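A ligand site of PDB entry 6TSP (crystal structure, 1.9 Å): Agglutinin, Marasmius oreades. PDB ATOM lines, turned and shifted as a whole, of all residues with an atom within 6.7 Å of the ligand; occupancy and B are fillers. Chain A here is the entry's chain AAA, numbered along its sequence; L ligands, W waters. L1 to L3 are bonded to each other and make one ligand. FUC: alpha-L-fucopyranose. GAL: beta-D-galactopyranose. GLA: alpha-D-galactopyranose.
N of Thr 38 sits at hydrogen-bond distance from O3 of GLA L3 (3.1 Å).
O6 of GAL L2 is in hydrogen-bond range of OD1 of Asp 20 (2.5 Å).
O6 of GAL L2 is in hydrogen-bond range of N of Asp 23 (2.7 Å).
An oxygen (O5) of GAL L2 sits at hydrogen-bond distance from a ring nitrogen (ND1) of His 45 (2.9 Å).
O of Gln 36 lies within hydrogen-bond range of O4 of GLA L3 (3.4 Å).
The side-chain amide oxygen of Asn 43 is in hydrogen-bond range of an oxygen (O2) of GLA L3, 3.0 Å away.
An oxygen (O3) of GLA L3 sits at hydrogen-bond distance from the side-chain hydroxyl (OG1) of Thr 38.
The indole nitrogen (NE1) of Trp 35 lies within hydrogen-bond range of an oxygen (O6) of GLA L3, 3.0 Å away.
The backbone carbonyl oxygen (O) of His 45 lies within hydrogen-bond range of the backbone NH (N) of Leu 21 (3.0 Å).
O of Gln 36 sits at hydrogen-bond distance from NE2 of Gln 46 (3.1 Å).
OE1 of Gln 46 sits at hydrogen-bond distance from NE2 of His 9 (2.6 Å).
The backbone NH of Thr 38 lies within hydrogen-bond range of the side-chain amide oxygen of Asn 43 (3.1 Å).
NE2 of Gln 36 sits at hydrogen-bond distance from OD2 of Asp 131 (2.7 Å).
NE2 of Gln 46 lies within hydrogen-bond range of OD2 of Asp 20 (2.9 Å).
The backbone carbonyl oxygen (O) of Thr 38 is in hydrogen-bond range of the side-chain hydroxyl (OG1) of Thr 41 (2.7 Å).
The backbone NH (N) of Val 33 is in hydrogen-bond range of the backbone carbonyl oxygen (O) of Asp 20 (2.8 Å).
Merely in contact with the ligand: Leu 21 (3.6 Å), Lys 22 (3.5 Å), Phe 37 (3.6 Å), Trp 44 (3.98 Å) and Gln 46 (3.8 Å).
The nearest printed residue that does not touch the ligand is Gly 24 (4.2 Å).
Water W4 lies within hydrogen-bond range of O3 of GLA L3, OG1 of Thr 41, O of Ile 42 and OD1 of Asn 43.
Water W5 lies within hydrogen-bond range of O2 of GLA L3 (2.6 Å), N of His 45 (2.9 Å) and N of Trp 44 (3.0 Å).
Water W1 lies within hydrogen-bond range of an oxygen (O2) of GLA L3 (2.8 Å), the backbone NH (N) of Trp 44 (3.0 Å) and the backbone carbonyl oxygen (O) of Ile 42 (3.2 Å).
Water W6 lies within hydrogen-bond range of OD1 of Asp 23 (2.8 Å) and O5 of GAL L2 (2.9 Å).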
ATOM      1  N   HIS A   9     -16.123  23.489 -20.213  1.00  0.00           N
ATOM      2  CA  HIS A   9     -16.273  23.308 -21.656  1.00  0.00           C
ATOM      3  C   HIS A   9     -17.659  23.818 -22.086  1.00  0.00           C
ATOM      4  O   HIS A   9     -18.668  23.324 -21.558  1.00  0.00           O
ATOM      5  CB  HIS A   9     -16.059  21.813 -22.022  1.00  0.00           C
ATOM      6  CG  HIS A   9     -15.873  21.577 -23.479  1.00  0.00           C
ATOM      7  ND1 HIS A   9     -16.802  20.865 -24.238  1.00  0.00           N
ATOM      8  CD2 HIS A   9     -14.879  21.937 -24.330  1.00  0.00           C
ATOM      9  CE1 HIS A   9     -16.415  20.853 -25.501  1.00  0.00           C
ATOM     10  NE2 HIS A   9     -15.210  21.442 -25.567  1.00  0.00           N
ATOM     11  N   ASP A  20     -14.348  28.173 -28.759  1.00  0.00           N
ATOM     12  CA  ASP A  20     -12.985  27.755 -29.150  1.00  0.00           C
ATOM     13  C   ASP A  20     -12.148  29.008 -29.451  1.00  0.00           C
ATOM     14  O   ASP A  20     -12.598  29.838 -30.280  1.00  0.00           O
ATOM     15  CB  ASP A  20     -13.017  26.794 -30.352  1.00  0.00           C
ATOM     16  CG  ASP A  20     -11.662  26.170 -30.718  1.00  0.00           C
ATOM     17  OD1 ASP A  20     -10.752  26.938 -31.166  1.00  0.00           O
ATOM     18  OD2 ASP A  20     -11.577  24.918 -30.698  1.00  0.00           O
ATOM     19  N   LEU A  21     -11.079  29.218 -28.696  1.00  0.00           N
ATOM     20  CA  LEU A  21     -10.081  30.253 -29.024  1.00  0.00           C
ATOM     21  C   LEU A  21      -9.202  29.741 -30.152  1.00  0.00           C
ATOM     22  O   LEU A  21      -8.506  28.708 -29.939  1.00  0.00           O
ATOM     23  CB  LEU A  21      -9.245  30.569 -27.770  1.00  0.00           C
ATOM     24  CG  LEU A  21      -8.145  31.615 -27.966  1.00  0.00           C
ATOM     25  CD1 LEU A  21      -8.738  32.905 -28.494  1.00  0.00           C
ATOM     26  CD2 LEU A  21      -7.396  31.862 -26.665  1.00  0.00           C
ATOM     27  N   LYS A  22      -9.310  30.343 -31.345  1.00  0.00           N
ATOM     28  CA  LYS A  22      -8.852  29.714 -32.615  1.00  0.00           C
ATOM     29  C   LYS A  22      -7.333  29.467 -32.551  1.00  0.00           C
ATOM     30  O   LYS A  22      -6.584  30.417 -32.171  1.00  0.00           O
ATOM     31  CB  LYS A  22      -9.199  30.570 -33.836  1.00  0.00           C
ATOM     32  CG  LYS A  22      -9.280  29.792 -35.134  1.00  0.00           C
ATOM     33  CD  LYS A  22      -9.707  30.592 -36.336  1.00  0.00           C
ATOM     34  CE  LYS A  22      -9.758  29.743 -37.588  1.00  0.00           C
ATOM     35  NZ  LYS A  22     -10.260  30.506 -38.756  1.00  0.00           N
ATOM     36  N   ASP A  23      -6.930  28.210 -32.738  1.00  0.00           N
ATOM     37  CA  ASP A  23      -5.518  27.748 -32.662  1.00  0.00           C
ATOM     38  C   ASP A  23      -4.928  28.031 -31.276  1.00  0.00           C
ATOM     39  O   ASP A  23      -3.700  27.820 -31.101  1.00  0.00           O
ATOM     40  CB  ASP A  23      -4.655  28.380 -33.743  1.00  0.00           C
ATOM     41  CG  ASP A  23      -3.442  27.548 -34.116  1.00  0.00           C
ATOM     42  OD1 ASP A  23      -3.582  26.301 -34.170  1.00  0.00           O
ATOM     43  OD2 ASP A  23      -2.357  28.127 -34.301  1.00  0.00           O
ATOM     44  N   GLY A  24      -5.776  28.350 -30.308  1.00  0.00           N
ATOM     45  CA  GLY A  24      -5.351  28.570 -28.921  1.00  0.00           C
ATOM     46  C   GLY A  24      -4.301  29.680 -28.827  1.00  0.00           C
ATOM     47  O   GLY A  24      -3.604  29.740 -27.803  1.00  0.00           O
ATOM     48  N   VAL A  33     -14.541  31.214 -31.705  1.00  0.00           N
ATOM     49  CA  VAL A  33     -15.376  30.617 -32.772  1.00  0.00           C
ATOM     50  C   VAL A  33     -16.081  29.392 -32.204  1.00  0.00           C
ATOM     51  O   VAL A  33     -15.553  28.796 -31.229  1.00  0.00           O
ATOM     52  CB  VAL A  33     -14.535  30.249 -34.028  1.00  0.00           C
ATOM     53  CG1 VAL A  33     -14.002  31.481 -34.720  1.00  0.00           C
ATOM     54  CG2 VAL A  33     -13.398  29.272 -33.689  1.00  0.00           C
ATOM     55  N   TRP A  35     -16.581  25.358 -32.672  1.00  0.00           N
ATOM     56  CA  TRP A  35     -15.741  24.249 -33.160  1.00  0.00           C
ATOM     57  C   TRP A  35     -16.209  22.928 -32.529  1.00  0.00           C
ATOM     58  O   TRP A  35     -16.508  22.928 -31.320  1.00  0.00           O
ATOM     59  CB  TRP A  35     -14.259  24.529 -32.854  1.00  0.00           C
ATOM     60  CG  TRP A  35     -13.333  23.887 -33.825  1.00  0.00           C
ATOM     61  CD1 TRP A  35     -13.025  22.555 -33.912  1.00  0.00           C
ATOM     62  CD2 TRP A  35     -12.653  24.529 -34.909  1.00  0.00           C
ATOM     63  NE1 TRP A  35     -12.139  22.341 -34.931  1.00  0.00           N
ATOM     64  CE2 TRP A  35     -11.899  23.527 -35.579  1.00  0.00           C
ATOM     65  CE3 TRP A  35     -12.579  25.848 -35.365  1.00  0.00           C
ATOM     66  CZ2 TRP A  35     -11.094  23.811 -36.676  1.00  0.00           C
ATOM     67  CZ3 TRP A  35     -11.793  26.125 -36.473  1.00  0.00           C
ATOM     68  CH2 TRP A  35     -11.050  25.119 -37.104  1.00  0.00           C
ATOM     69  N   GLN A  36     -16.226  21.866 -33.323  1.00  0.00           N
ATOM     70  CA  GLN A  36     -16.643  20.544 -32.861  1.00  0.00           C
ATOM     71  C   GLN A  36     -15.607  20.022 -31.870  1.00  0.00           C
ATOM     72  O   GLN A  36     -14.527  20.676 -31.737  1.00  0.00           O
ATOM     73  CB  GLN A  36     -16.829  19.570 -34.063  1.00  0.00           C
ATOM     74  CG  GLN A  36     -15.533  19.116 -34.717  1.00  0.00           C
ATOM     75  CD  GLN A  36     -15.780  18.174 -35.883  1.00  0.00           C
ATOM     76  OE1 GLN A  36     -16.206  17.034 -35.690  1.00  0.00           O
ATOM     77  NE2 GLN A  36     -15.653  18.693 -37.106  1.00  0.00           N
ATOM     78  N   PHE A  37     -15.997  19.103 -31.056  1.00  0.00           N
ATOM     79  CA  PHE A  37     -15.200  18.662 -29.885  1.00  0.00           C
ATOM     80  C   PHE A  37     -15.274  17.141 -29.782  1.00  0.00           C
ATOM     81  O   PHE A  37     -16.158  16.519 -30.426  1.00  0.00           O
ATOM     82  CB  PHE A  37     -15.708  19.337 -28.617  1.00  0.00           C
ATOM     83  CG  PHE A  37     -17.187  19.222 -28.384  1.00  0.00           C
ATOM     84  CD1 PHE A  37     -18.042  20.220 -28.799  1.00  0.00           C
ATOM     85  CD2 PHE A  37     -17.690  18.240 -27.538  1.00  0.00           C
ATOM     86  CE1 PHE A  37     -19.406  20.154 -28.506  1.00  0.00           C
ATOM     87  CE2 PHE A  37     -19.039  18.200 -27.221  1.00  0.00           C
ATOM     88  CZ  PHE A  37     -19.891  19.132 -27.745  1.00  0.00           C
ATOM     89  N   THR A  38     -14.347  16.556 -29.047  1.00  0.00           N
ATOM     90  CA  THR A  38     -14.365  15.110 -28.731  1.00  0.00           C
ATOM     91  C   THR A  38     -14.567  14.933 -27.222  1.00  0.00           C
ATOM     92  O   THR A  38     -13.763  15.411 -26.428  1.00  0.00           O
ATOM     93  CB  THR A  38     -13.072  14.440 -29.230  1.00  0.00           C
ATOM     94  OG1 THR A  38     -12.848  14.835 -30.581  1.00  0.00           O
ATOM     95  CG2 THR A  38     -13.115  12.937 -29.132  1.00  0.00           C
ATOM     96  N   PRO A  39     -15.640  14.237 -26.795  1.00  0.00           N
ATOM     97  CA  PRO A  39     -15.877  13.985 -25.371  1.00  0.00           C
ATOM     98  C   PRO A  39     -14.796  13.094 -24.744  1.00  0.00           C
ATOM     99  O   PRO A  39     -14.240  12.280 -25.435  1.00  0.00           O
ATOM    100  CB  PRO A  39     -17.235  13.235 -25.339  1.00  0.00           C
ATOM    101  CG  PRO A  39     -17.835  13.474 -26.735  1.00  0.00           C
ATOM    102  CD  PRO A  39     -16.645  13.638 -27.648  1.00  0.00           C
ATOM    103  N   THR A  41     -11.947  13.773 -23.876  1.00  0.00           N
ATOM    104  CA  THR A  41     -10.557  14.219 -24.147  1.00  0.00           C
ATOM    105  C   THR A  41     -10.294  15.504 -23.399  1.00  0.00           C
ATOM    106  O   THR A  41     -11.281  16.173 -22.986  1.00  0.00           O
ATOM    107  CB  THR A  41     -10.286  14.407 -25.649  1.00  0.00           C
ATOM    108  OG1 THR A  41     -11.041  15.550 -26.086  1.00  0.00           O
ATOM    109  CG2 THR A  41     -10.660  13.207 -26.479  1.00  0.00           C
ATOM    110  N   ILE A  42      -9.065  15.956 -23.450  1.00  0.00           N
ATOM    111  CA  ILE A  42      -8.723  17.368 -23.286  1.00  0.00           C
ATOM    112  C   ILE A  42      -9.000  18.080 -24.616  1.00  0.00           C
ATOM    113  O   ILE A  42      -8.317  17.771 -25.599  1.00  0.00           O
ATOM    114  CB  ILE A  42      -7.248  17.500 -22.856  1.00  0.00           C
ATOM    115  CG1 ILE A  42      -6.985  16.828 -21.508  1.00  0.00           C
ATOM    116  CG2 ILE A  42      -6.828  18.957 -22.852  1.00  0.00           C
ATOM    117  CD1 ILE A  42      -7.824  17.392 -20.351  1.00  0.00           C
ATOM    118  N   ASN A  43      -9.965  18.990 -24.626  1.00  0.00           N
ATOM    119  CA  ASN A  43     -10.200  19.908 -25.798  1.00  0.00           C
ATOM    120  C   ASN A  43      -9.372  21.169 -25.592  1.00  0.00           C
ATOM    121  O   ASN A  43      -9.832  22.108 -24.845  1.00  0.00           O
ATOM    122  CB  ASN A  43     -11.673  20.202 -26.007  1.00  0.00           C
ATOM    123  CG  ASN A  43     -12.458  18.957 -26.362  1.00  0.00           C
ATOM    124  OD1 ASN A  43     -12.408  18.487 -27.500  1.00  0.00           O
ATOM    125  ND2 ASN A  43     -13.134  18.379 -25.364  1.00  0.00           N
ATOM    126  N   TRP A  44      -8.196  21.209 -26.197  1.00  0.00           N
ATOM    127  CA  TRP A  44      -7.061  22.024 -25.739  1.00  0.00           C
ATOM    128  C   TRP A  44      -7.411  23.529 -25.825  1.00  0.00           C
ATOM    129  O   TRP A  44      -6.839  24.326 -25.027  1.00  0.00           O
ATOM    130  CB  TRP A  44      -5.827  21.691 -26.549  1.00  0.00           C
ATOM    131  CG  TRP A  44      -5.071  20.541 -25.995  1.00  0.00           C
ATOM    132  CD1 TRP A  44      -5.119  19.245 -26.407  1.00  0.00           C
ATOM    133  CD2 TRP A  44      -4.224  20.555 -24.840  1.00  0.00           C
ATOM    134  NE1 TRP A  44      -4.337  18.464 -25.610  1.00  0.00           N
ATOM    135  CE2 TRP A  44      -3.773  19.237 -24.643  1.00  0.00           C
ATOM    136  CE3 TRP A  44      -3.776  21.560 -23.981  1.00  0.00           C
ATOM    137  CZ2 TRP A  44      -2.898  18.900 -23.616  1.00  0.00           C
ATOM    138  CZ3 TRP A  44      -2.941  21.226 -22.943  1.00  0.00           C
ATOM    139  CH2 TRP A  44      -2.497  19.913 -22.773  1.00  0.00           C
ATOM    140  N   HIS A  45      -8.209  23.924 -26.826  1.00  0.00           N
ATOM    141  CA  HIS A  45      -8.473  25.359 -27.124  1.00  0.00           C
ATOM    142  C   HIS A  45      -9.836  25.774 -26.570  1.00  0.00           C
ATOM    143  O   HIS A  45     -10.237  27.007 -26.779  1.00  0.00           O
ATOM    144  CB  HIS A  45      -8.361  25.616 -28.633  1.00  0.00           C
ATOM    145  CG  HIS A  45      -7.029  25.276 -29.188  1.00  0.00           C
ATOM    146  ND1 HIS A  45      -6.831  25.003 -30.537  1.00  0.00           N
ATOM    147  CD2 HIS A  45      -5.831  25.097 -28.585  1.00  0.00           C
ATOM    148  CE1 HIS A  45      -5.554  24.686 -30.726  1.00  0.00           C
ATOM    149  NE2 HIS A  45      -4.941  24.690 -29.535  1.00  0.00           N
ATOM    150  N   GLN A  46     -10.479  24.900 -25.809  1.00  0.00           N
ATOM    151  CA  GLN A  46     -11.957  24.973 -25.537  1.00  0.00           C
ATOM    152  C   GLN A  46     -12.248  24.926 -24.012  1.00  0.00           C
ATOM    153  O   GLN A  46     -13.389  24.611 -23.641  1.00  0.00           O
ATOM    154  CB  GLN A  46     -12.676  23.844 -26.251  1.00  0.00           C
ATOM    155  CG  GLN A  46     -12.674  23.971 -27.754  1.00  0.00           C
ATOM    156  CD  GLN A  46     -13.331  22.780 -28.436  1.00  0.00           C
ATOM    157  OE1 GLN A  46     -13.871  21.890 -27.779  1.00  0.00           O
ATOM    158  NE2 GLN A  46     -13.301  22.767 -29.771  1.00  0.00           N
ATOM    159  N   PHE A  66      -5.676  27.450 -21.874  1.00  0.00           N
ATOM    160  CA  PHE A  66      -4.465  27.190 -22.681  1.00  0.00           C
ATOM    161  C   PHE A  66      -3.713  28.506 -22.934  1.00  0.00           C
ATOM    162  O   PHE A  66      -2.471  28.529 -22.767  1.00  0.00           O
ATOM    163  CB  PHE A  66      -4.830  26.517 -23.999  1.00  0.00           C
ATOM    164  CG  PHE A  66      -3.641  26.198 -24.870  1.00  0.00           C
ATOM    165  CD1 PHE A  66      -2.728  25.209 -24.490  1.00  0.00           C
ATOM    166  CD2 PHE A  66      -3.369  26.945 -26.024  1.00  0.00           C
ATOM    167  CE1 PHE A  66      -1.609  24.946 -25.281  1.00  0.00           C
ATOM    168  CE2 PHE A  66      -2.246  26.680 -26.801  1.00  0.00           C
ATOM    169  CZ  PHE A  66      -1.367  25.676 -26.431  1.00  0.00           C
ATOM    170  N   ASP A 131     -16.952  24.399 -38.316  1.00  0.00           N
ATOM    171  CA  ASP A 131     -15.711  24.661 -37.560  1.00  0.00           C
ATOM    172  C   ASP A 131     -15.163  26.041 -37.964  1.00  0.00           C
ATOM    173  O   ASP A 131     -14.950  26.249 -39.137  1.00  0.00           O
ATOM    174  CB  ASP A 131     -14.698  23.545 -37.783  1.00  0.00           C
ATOM    175  CG  ASP A 131     -15.078  22.227 -37.100  1.00  0.00           C
ATOM    176  OD1 ASP A 131     -15.904  22.278 -36.199  1.00  0.00           O
ATOM    177  OD2 ASP A 131     -14.590  21.171 -37.548  1.00  0.00           O
HETATM  178  C1  FUC L   1      -6.821  19.483 -31.940  1.00  0.00           C
HETATM  179  C2  FUC L   1      -6.229  18.271 -32.583  1.00  0.00           C
HETATM  180  C3  FUC L   1      -4.769  18.498 -32.946  1.00  0.00           C
HETATM  181  C4  FUC L   1      -3.984  19.073 -31.760  1.00  0.00           C
HETATM  182  C5  FUC L   1      -4.696  20.302 -31.209  1.00  0.00           C
HETATM  183  C6  FUC L   1      -3.980  20.920 -29.990  1.00  0.00           C
HETATM  184  O2  FUC L   1      -6.967  17.967 -33.779  1.00  0.00           O
HETATM  185  O3  FUC L   1      -4.225  17.264 -33.329  1.00  0.00           O
HETATM  186  O4  FUC L   1      -3.843  18.088 -30.753  1.00  0.00           O
HETATM  187  O5  FUC L   1      -6.025  19.926 -30.838  1.00  0.00           O
HETATM  188  C1  GAL L   2      -6.869  22.760 -33.476  1.00  0.00           C
HETATM  189  C2  GAL L   2      -7.486  21.728 -32.550  1.00  0.00           C
HETATM  190  C3  GAL L   2      -9.030  21.684 -32.688  1.00  0.00           C
HETATM  191  C4  GAL L   2      -9.580  23.112 -32.514  1.00  0.00           C
HETATM  192  C5  GAL L   2      -8.848  24.033 -33.533  1.00  0.00           C
HETATM  193  C6  GAL L   2      -9.364  25.473 -33.537  1.00  0.00           C
HETATM  194  O1  GAL L   2      -5.481  22.810 -33.186  1.00  0.00           O
HETATM  195  O2  GAL L   2      -6.931  20.472 -32.858  1.00  0.00           O
HETATM  196  O3  GAL L   2      -9.527  20.801 -31.759  1.00  0.00           O
HETATM  197  O4  GAL L   2      -9.452  23.591 -31.154  1.00  0.00           O
HETATM  198  O5  GAL L   2      -7.444  24.031 -33.249  1.00  0.00           O
HETATM  199  O6  GAL L   2      -8.708  26.257 -32.503  1.00  0.00           O
HETATM  200  C1  GLA L   3     -10.883  20.575 -31.695  1.00  0.00           C
HETATM  201  C2  GLA L   3     -11.268  19.556 -30.618  1.00  0.00           C
HETATM  202  C3  GLA L   3     -10.907  18.094 -31.046  1.00  0.00           C
HETATM  203  C4  GLA L   3     -11.412  17.835 -32.449  1.00  0.00           C
HETATM  204  C5  GLA L   3     -10.857  18.915 -33.374  1.00  0.00           C
HETATM  205  C6  GLA L   3     -11.204  18.658 -34.846  1.00  0.00           C
HETATM  206  O2  GLA L   3     -10.610  19.908 -29.408  1.00  0.00           O
HETATM  207  O3  GLA L   3     -11.471  17.161 -30.138  1.00  0.00           O
HETATM  208  O4  GLA L   3     -12.860  17.816 -32.481  1.00  0.00           O
HETATM  209  O5  GLA L   3     -11.396  20.156 -32.976  1.00  0.00           O
HETATM  210  O6  GLA L   3     -10.756  19.780 -35.633  1.00  0.00           O
HETATM  211  O   HOH W   1      -8.038  19.169 -28.433  1.00  0.00           O
HETATM  212  O   HOH W   2      -1.532  17.559 -29.275  1.00  0.00           O
HETATM  213  O   HOH W   3      -7.877  19.598 -35.713  1.00  0.00           O
HETATM  214  O   HOH W   4      -9.783  16.814 -28.188  1.00  0.00           O
HETATM  215  O   HOH W   5      -9.443  22.164 -28.746  1.00  0.00           O
HETATM  216  O   HOH W   6      -6.052  25.577 -35.225  1.00  0.00           O
